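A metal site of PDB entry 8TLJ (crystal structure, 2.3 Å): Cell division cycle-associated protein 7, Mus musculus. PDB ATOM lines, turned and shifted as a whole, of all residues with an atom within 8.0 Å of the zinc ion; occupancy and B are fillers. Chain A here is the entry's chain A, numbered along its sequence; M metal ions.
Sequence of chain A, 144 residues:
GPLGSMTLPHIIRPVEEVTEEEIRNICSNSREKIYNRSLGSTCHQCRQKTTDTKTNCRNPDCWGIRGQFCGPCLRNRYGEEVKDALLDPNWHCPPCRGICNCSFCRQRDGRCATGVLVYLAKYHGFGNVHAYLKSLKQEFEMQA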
ATOM      1  N   HIS A  44       3.949  -5.733 -14.941  1.00  0.00           N
ATOM      2  CA  HIS A  44       3.373  -5.251 -13.689  1.00  0.00           C
ATOM      3  C   HIS A  44       4.456  -4.834 -12.698  1.00  0.00           C
ATOM      4  O   HIS A  44       4.289  -3.845 -11.969  1.00  0.00           O
ATOM      5  CB  HIS A  44       2.482  -6.319 -13.064  1.00  0.00           C
ATOM      6  CG  HIS A  44       2.015  -5.980 -11.677  1.00  0.00           C
ATOM      7  ND1 HIS A  44       1.086  -4.985 -11.433  1.00  0.00           N
ATOM      8  CD2 HIS A  44       2.367  -6.478 -10.474  1.00  0.00           C
ATOM      9  CE1 HIS A  44       0.880  -4.906 -10.125  1.00  0.00           C
ATOM     10  NE2 HIS A  44       1.643  -5.799  -9.529  1.00  0.00           N
ATOM     11  N   GLN A  45       5.574  -5.555 -12.674  1.00  0.00           N
ATOM     12  CA  GLN A  45       6.607  -5.308 -11.657  1.00  0.00           C
ATOM     13  C   GLN A  45       7.328  -3.991 -11.916  1.00  0.00           C
ATOM     14  O   GLN A  45       7.300  -3.084 -11.071  1.00  0.00           O
ATOM     15  CB  GLN A  45       7.602  -6.478 -11.632  1.00  0.00           C
ATOM     16  CG  GLN A  45       8.605  -6.415 -10.486  1.00  0.00           C
ATOM     17  CD  GLN A  45       8.042  -6.960  -9.182  1.00  0.00           C
ATOM     18  OE1 GLN A  45       7.029  -7.657  -9.173  1.00  0.00           O
ATOM     19  NE2 GLN A  45       8.696  -6.635  -8.072  1.00  0.00           N
ATOM     20  N   ARG A  47       6.724  -1.869 -14.449  1.00  0.00           N
ATOM     21  CA  ARG A  47       5.812  -0.868 -15.013  1.00  0.00           C
ATOM     22  C   ARG A  47       6.403  -0.183 -16.242  1.00  0.00           C
ATOM     23  O   ARG A  47       6.223   1.016 -16.462  1.00  0.00           O
ATOM     24  CB  ARG A  47       5.406   0.160 -13.950  1.00  0.00           C
ATOM     25  CG  ARG A  47       4.825  -0.495 -12.689  1.00  0.00           C
ATOM     26  CD  ARG A  47       4.172   0.514 -11.764  1.00  0.00           C
ATOM     27  NE  ARG A  47       5.140   1.326 -11.038  1.00  0.00           N
ATOM     28  CZ  ARG A  47       5.634   1.017  -9.844  1.00  0.00           C
ATOM     29  NH1 ARG A  47       5.265  -0.094  -9.216  1.00  0.00           N
ATOM     30  NH2 ARG A  47       6.497   1.837  -9.270  1.00  0.00           N
ATOM     31  N   ARG A  66      -2.242  -7.147 -14.531  1.00  0.00           N
ATOM     32  CA  ARG A  66      -1.518  -7.478 -13.305  1.00  0.00           C
ATOM     33  C   ARG A  66      -0.725  -8.770 -13.439  1.00  0.00           C
ATOM     34  O   ARG A  66       0.231  -8.970 -12.690  1.00  0.00           O
ATOM     35  CB  ARG A  66      -2.503  -7.596 -12.130  1.00  0.00           C
ATOM     36  CG  ARG A  66      -3.424  -8.803 -12.219  1.00  0.00           C
ATOM     37  CD  ARG A  66      -4.712  -8.584 -11.444  1.00  0.00           C
ATOM     38  NE  ARG A  66      -4.515  -8.583 -10.003  1.00  0.00           N
ATOM     39  CZ  ARG A  66      -4.542  -9.670  -9.239  1.00  0.00           C
ATOM     40  NH1 ARG A  66      -4.718 -10.871  -9.765  1.00  0.00           N
ATOM     41  NH2 ARG A  66      -4.375  -9.555  -7.933  1.00  0.00           N
ATOM     42  N   PHE A  69       4.399 -10.131 -16.726  1.00  0.00           N
ATOM     43  CA  PHE A  69       5.722  -9.922 -16.160  1.00  0.00           C
ATOM     44  C   PHE A  69       6.795 -10.156 -17.216  1.00  0.00           C
ATOM     45  O   PHE A  69       6.712 -11.112 -18.000  1.00  0.00           O
ATOM     46  CB  PHE A  69       5.972 -10.848 -14.957  1.00  0.00           C
ATOM     47  CG  PHE A  69       5.202 -10.471 -13.729  1.00  0.00           C
ATOM     48  CD1 PHE A  69       3.857 -10.789 -13.603  1.00  0.00           C
ATOM     49  CD2 PHE A  69       5.828  -9.797 -12.694  1.00  0.00           C
ATOM     50  CE1 PHE A  69       3.148 -10.440 -12.474  1.00  0.00           C
ATOM     51  CE2 PHE A  69       5.120  -9.439 -11.561  1.00  0.00           C
ATOM     52  CZ  PHE A  69       3.780  -9.761 -11.451  1.00  0.00           C
ATOM     53  N   TYR A  78      11.130 -13.393  -8.480  1.00  0.00           N
ATOM     54  CA  TYR A  78      10.355 -14.579  -8.137  1.00  0.00           C
ATOM     55  C   TYR A  78      11.052 -15.891  -8.463  1.00  0.00           C
ATOM     56  O   TYR A  78      10.490 -16.949  -8.153  1.00  0.00           O
ATOM     57  CB  TYR A  78       8.989 -14.522  -8.834  1.00  0.00           C
ATOM     58  CG  TYR A  78       8.223 -13.261  -8.501  1.00  0.00           C
ATOM     59  CD1 TYR A  78       7.530 -13.152  -7.300  1.00  0.00           C
ATOM     60  CD2 TYR A  78       8.233 -12.165  -9.360  1.00  0.00           C
ATOM     61  CE1 TYR A  78       6.857 -11.995  -6.973  1.00  0.00           C
ATOM     62  CE2 TYR A  78       7.561 -10.999  -9.029  1.00  0.00           C
ATOM     63  CZ  TYR A  78       6.869 -10.930  -7.835  1.00  0.00           C
ATOM     64  OH  TYR A  78       6.189  -9.787  -7.499  1.00  0.00           O
ATOM     65  N   PRO A  94       2.000 -13.688  -9.633  1.00  0.00           N
ATOM     66  CA  PRO A  94       2.258 -13.456  -8.206  1.00  0.00           C
ATOM     67  C   PRO A  94       1.136 -12.671  -7.538  1.00  0.00           C
ATOM     68  O   PRO A  94       0.772 -12.990  -6.392  1.00  0.00           O
ATOM     69  CB  PRO A  94       3.573 -12.662  -8.218  1.00  0.00           C
ATOM     70  CG  PRO A  94       4.266 -13.141  -9.447  1.00  0.00           C
ATOM     71  CD  PRO A  94       3.181 -13.406 -10.462  1.00  0.00           C
ATOM     72  N   PRO A  95       0.556 -11.649  -8.188  1.00  0.00           N
ATOM     73  CA  PRO A  95      -0.627 -11.011  -7.572  1.00  0.00           C
ATOM     74  C   PRO A  95      -1.776 -11.980  -7.311  1.00  0.00           C
ATOM     75  O   PRO A  95      -2.435 -11.889  -6.275  1.00  0.00           O
ATOM     76  CB  PRO A  95      -1.020  -9.927  -8.582  1.00  0.00           C
ATOM     77  CG  PRO A  95       0.258  -9.568  -9.228  1.00  0.00           C
ATOM     78  CD  PRO A  95       1.010 -10.860  -9.356  1.00  0.00           C
ATOM     79  N   ILE A  99       1.635 -12.944  -3.597  1.00  0.00           N
ATOM     80  CA  ILE A  99       3.032 -12.885  -3.179  1.00  0.00           C
ATOM     81  C   ILE A  99       3.783 -11.822  -3.970  1.00  0.00           C
ATOM     82  O   ILE A  99       5.018 -11.828  -4.009  1.00  0.00           O
ATOM     83  CB  ILE A  99       3.709 -14.261  -3.325  1.00  0.00           C
ATOM     84  CG1 ILE A  99       3.737 -14.668  -4.803  1.00  0.00           C
ATOM     85  CG2 ILE A  99       3.007 -15.304  -2.487  1.00  0.00           C
ATOM     86  CD1 ILE A  99       4.644 -15.850  -5.089  1.00  0.00           C
ATOM     87  N   CYS A 100       3.056 -10.895  -4.601  1.00  0.00           N
ATOM     88  CA  CYS A 100       3.722  -9.857  -5.367  1.00  0.00           C
ATOM     89  C   CYS A 100       4.497  -8.928  -4.445  1.00  0.00           C
ATOM     90  O   CYS A 100       3.995  -8.494  -3.401  1.00  0.00           O
ATOM     91  CB  CYS A 100       2.696  -9.055  -6.187  1.00  0.00           C
ATOM     92  SG  CYS A 100       3.440  -7.923  -7.393  1.00  0.00           S
ATOM     93  N   ASN A 101       5.736  -8.607  -4.843  1.00  0.00           N
ATOM     94  CA  ASN A 101       6.597  -7.740  -4.046  1.00  0.00           C
ATOM     95  C   ASN A 101       6.936  -6.446  -4.790  1.00  0.00           C
ATOM     96  O   ASN A 101       7.975  -5.824  -4.501  1.00  0.00           O
ATOM     97  CB  ASN A 101       7.877  -8.466  -3.632  1.00  0.00           C
ATOM     98  CG  ASN A 101       8.652  -9.039  -4.810  1.00  0.00           C
ATOM     99  OD1 ASN A 101       9.182  -8.295  -5.630  1.00  0.00           O
ATOM    100  ND2 ASN A 101       8.731 -10.359  -4.874  1.00  0.00           N
ATOM    101  N   CYS A 102       6.094  -6.016  -5.718  1.00  0.00           N
ATOM    102  CA  CYS A 102       6.306  -4.737  -6.378  1.00  0.00           C
ATOM    103  C   CYS A 102       6.045  -3.602  -5.387  1.00  0.00           C
ATOM    104  O   CYS A 102       5.456  -3.782  -4.317  1.00  0.00           O
ATOM    105  CB  CYS A 102       5.414  -4.598  -7.609  1.00  0.00           C
ATOM    106  SG  CYS A 102       3.684  -4.174  -7.282  1.00  0.00           S
ATOM    107  N   SER A 103       6.504  -2.398  -5.763  1.00  0.00           N
ATOM    108  CA  SER A 103       6.428  -1.256  -4.849  1.00  0.00           C
ATOM    109  C   SER A 103       4.995  -0.932  -4.447  1.00  0.00           C
ATOM    110  O   SER A 103       4.785  -0.321  -3.388  1.00  0.00           O
ATOM    111  CB  SER A 103       7.071  -0.029  -5.494  1.00  0.00           C
ATOM    112  OG  SER A 103       6.300   0.445  -6.587  1.00  0.00           O
ATOM    113  N   PHE A 104       4.003  -1.317  -5.250  1.00  0.00           N
ATOM    114  CA  PHE A 104       2.608  -1.048  -4.902  1.00  0.00           C
ATOM    115  C   PHE A 104       2.002  -2.168  -4.058  1.00  0.00           C
ATOM    116  O   PHE A 104       1.346  -1.889  -3.055  1.00  0.00           O
ATOM    117  CB  PHE A 104       1.777  -0.860  -6.184  1.00  0.00           C
ATOM    118  CG  PHE A 104       0.302  -0.719  -5.932  1.00  0.00           C
ATOM    119  CD1 PHE A 104      -0.245   0.501  -5.571  1.00  0.00           C
ATOM    120  CD2 PHE A 104      -0.538  -1.817  -6.065  1.00  0.00           C
ATOM    121  CE1 PHE A 104      -1.599   0.630  -5.341  1.00  0.00           C
ATOM    122  CE2 PHE A 104      -1.898  -1.692  -5.823  1.00  0.00           C
ATOM    123  CZ  PHE A 104      -2.426  -0.470  -5.469  1.00  0.00           C
ATOM    124  N   CYS A 105       2.217  -3.425  -4.447  1.00  0.00           N
ATOM    125  CA  CYS A 105       1.520  -4.518  -3.775  1.00  0.00           C
ATOM    126  C   CYS A 105       2.059  -4.758  -2.368  1.00  0.00           C
ATOM    127  O   CYS A 105       1.298  -5.172  -1.486  1.00  0.00           O
ATOM    128  CB  CYS A 105       1.611  -5.787  -4.625  1.00  0.00           C
ATOM    129  SG  CYS A 105       0.580  -5.732  -6.118  1.00  0.00           S
ATOM    130  N   ARG A 106       3.355  -4.512  -2.139  1.00  0.00           N
ATOM    131  CA  ARG A 106       3.890  -4.606  -0.793  1.00  0.00           C
ATOM    132  C   ARG A 106       3.691  -3.318   0.006  1.00  0.00           C
ATOM    133  O   ARG A 106       3.927  -3.319   1.216  1.00  0.00           O
ATOM    134  CB  ARG A 106       5.381  -4.960  -0.831  1.00  0.00           C
ATOM    135  CG  ARG A 106       6.314  -3.819  -1.251  1.00  0.00           C
ATOM    136  CD  ARG A 106       7.764  -4.300  -1.341  1.00  0.00           C
ATOM    137  NE  ARG A 106       8.685  -3.195  -1.548  1.00  0.00           N
ATOM    138  CZ  ARG A 106       9.195  -2.841  -2.728  1.00  0.00           C
ATOM    139  NH1 ARG A 106       8.897  -3.512  -3.832  1.00  0.00           N
ATOM    140  NH2 ARG A 106      10.017  -1.800  -2.791  1.00  0.00           N
ATOM    141  N   GLN A 107       3.256  -2.242  -0.647  1.00  0.00           N
ATOM    142  CA  GLN A 107       3.014  -0.987   0.061  1.00  0.00           C
ATOM    143  C   GLN A 107       1.845  -1.115   1.038  1.00  0.00           C
ATOM    144  O   GLN A 107       1.930  -0.652   2.185  1.00  0.00           O
ATOM    145  CB  GLN A 107       2.751   0.137  -0.940  1.00  0.00           C
ATOM    146  CG  GLN A 107       3.658   1.346  -0.773  1.00  0.00           C
ATOM    147  CD  GLN A 107       3.374   2.422  -1.810  1.00  0.00           C
ATOM    148  OE1 GLN A 107       2.276   2.478  -2.375  1.00  0.00           O
ATOM    149  NE2 GLN A 107       4.362   3.262  -2.073  1.00  0.00           N
ATOM    150  N   ARG A 108       0.753  -1.720   0.591  1.00  0.00           N
ATOM    151  CA  ARG A 108      -0.458  -1.820   1.410  1.00  0.00           C
ATOM    152  C   ARG A 108      -0.365  -2.975   2.410  1.00  0.00           C
ATOM    153  O   ARG A 108       0.039  -4.082   2.068  1.00  0.00           O
ATOM    154  CB  ARG A 108      -1.687  -1.975   0.520  1.00  0.00           C
ATOM    155  CG  ARG A 108      -1.613  -3.163  -0.438  1.00  0.00           C
ATOM    156  CD  ARG A 108      -2.895  -3.338  -1.220  1.00  0.00           C
ATOM    157  NE  ARG A 108      -2.998  -4.681  -1.783  1.00  0.00           N
ATOM    158  CZ  ARG A 108      -2.483  -5.054  -2.946  1.00  0.00           C
ATOM    159  NH1 ARG A 108      -1.822  -4.192  -3.709  1.00  0.00           N
ATOM    160  NH2 ARG A 108      -2.627  -6.311  -3.346  1.00  0.00           N
HETATM  161 ZN    ZN M   1       2.288  -6.001  -7.594  1.00  0.00          ZN
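The side-chain sulfur (SG) of Cys 105 lies close to the guanidinium group (NH1) of Arg 108, 3.7 Å away.
The side-chain sulfur (SG) of Cys 100 sits close to the side-chain hydroxyl (OH) of Tyr 78 (3.3 Å).
NH1 of Arg 106 lies close to O of Cys 102 (3.5 Å).
SG of Cys 102 sits close to N of Phe 104, 3.5 Å away.
The nearest printed residue that does not touch the zinc ion is Pro 95 (4.4 Å).
The zinc ion is bound by NE2 of His 44, SG of Cys 100, SG of Cys 105 and SG of Cys 102.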
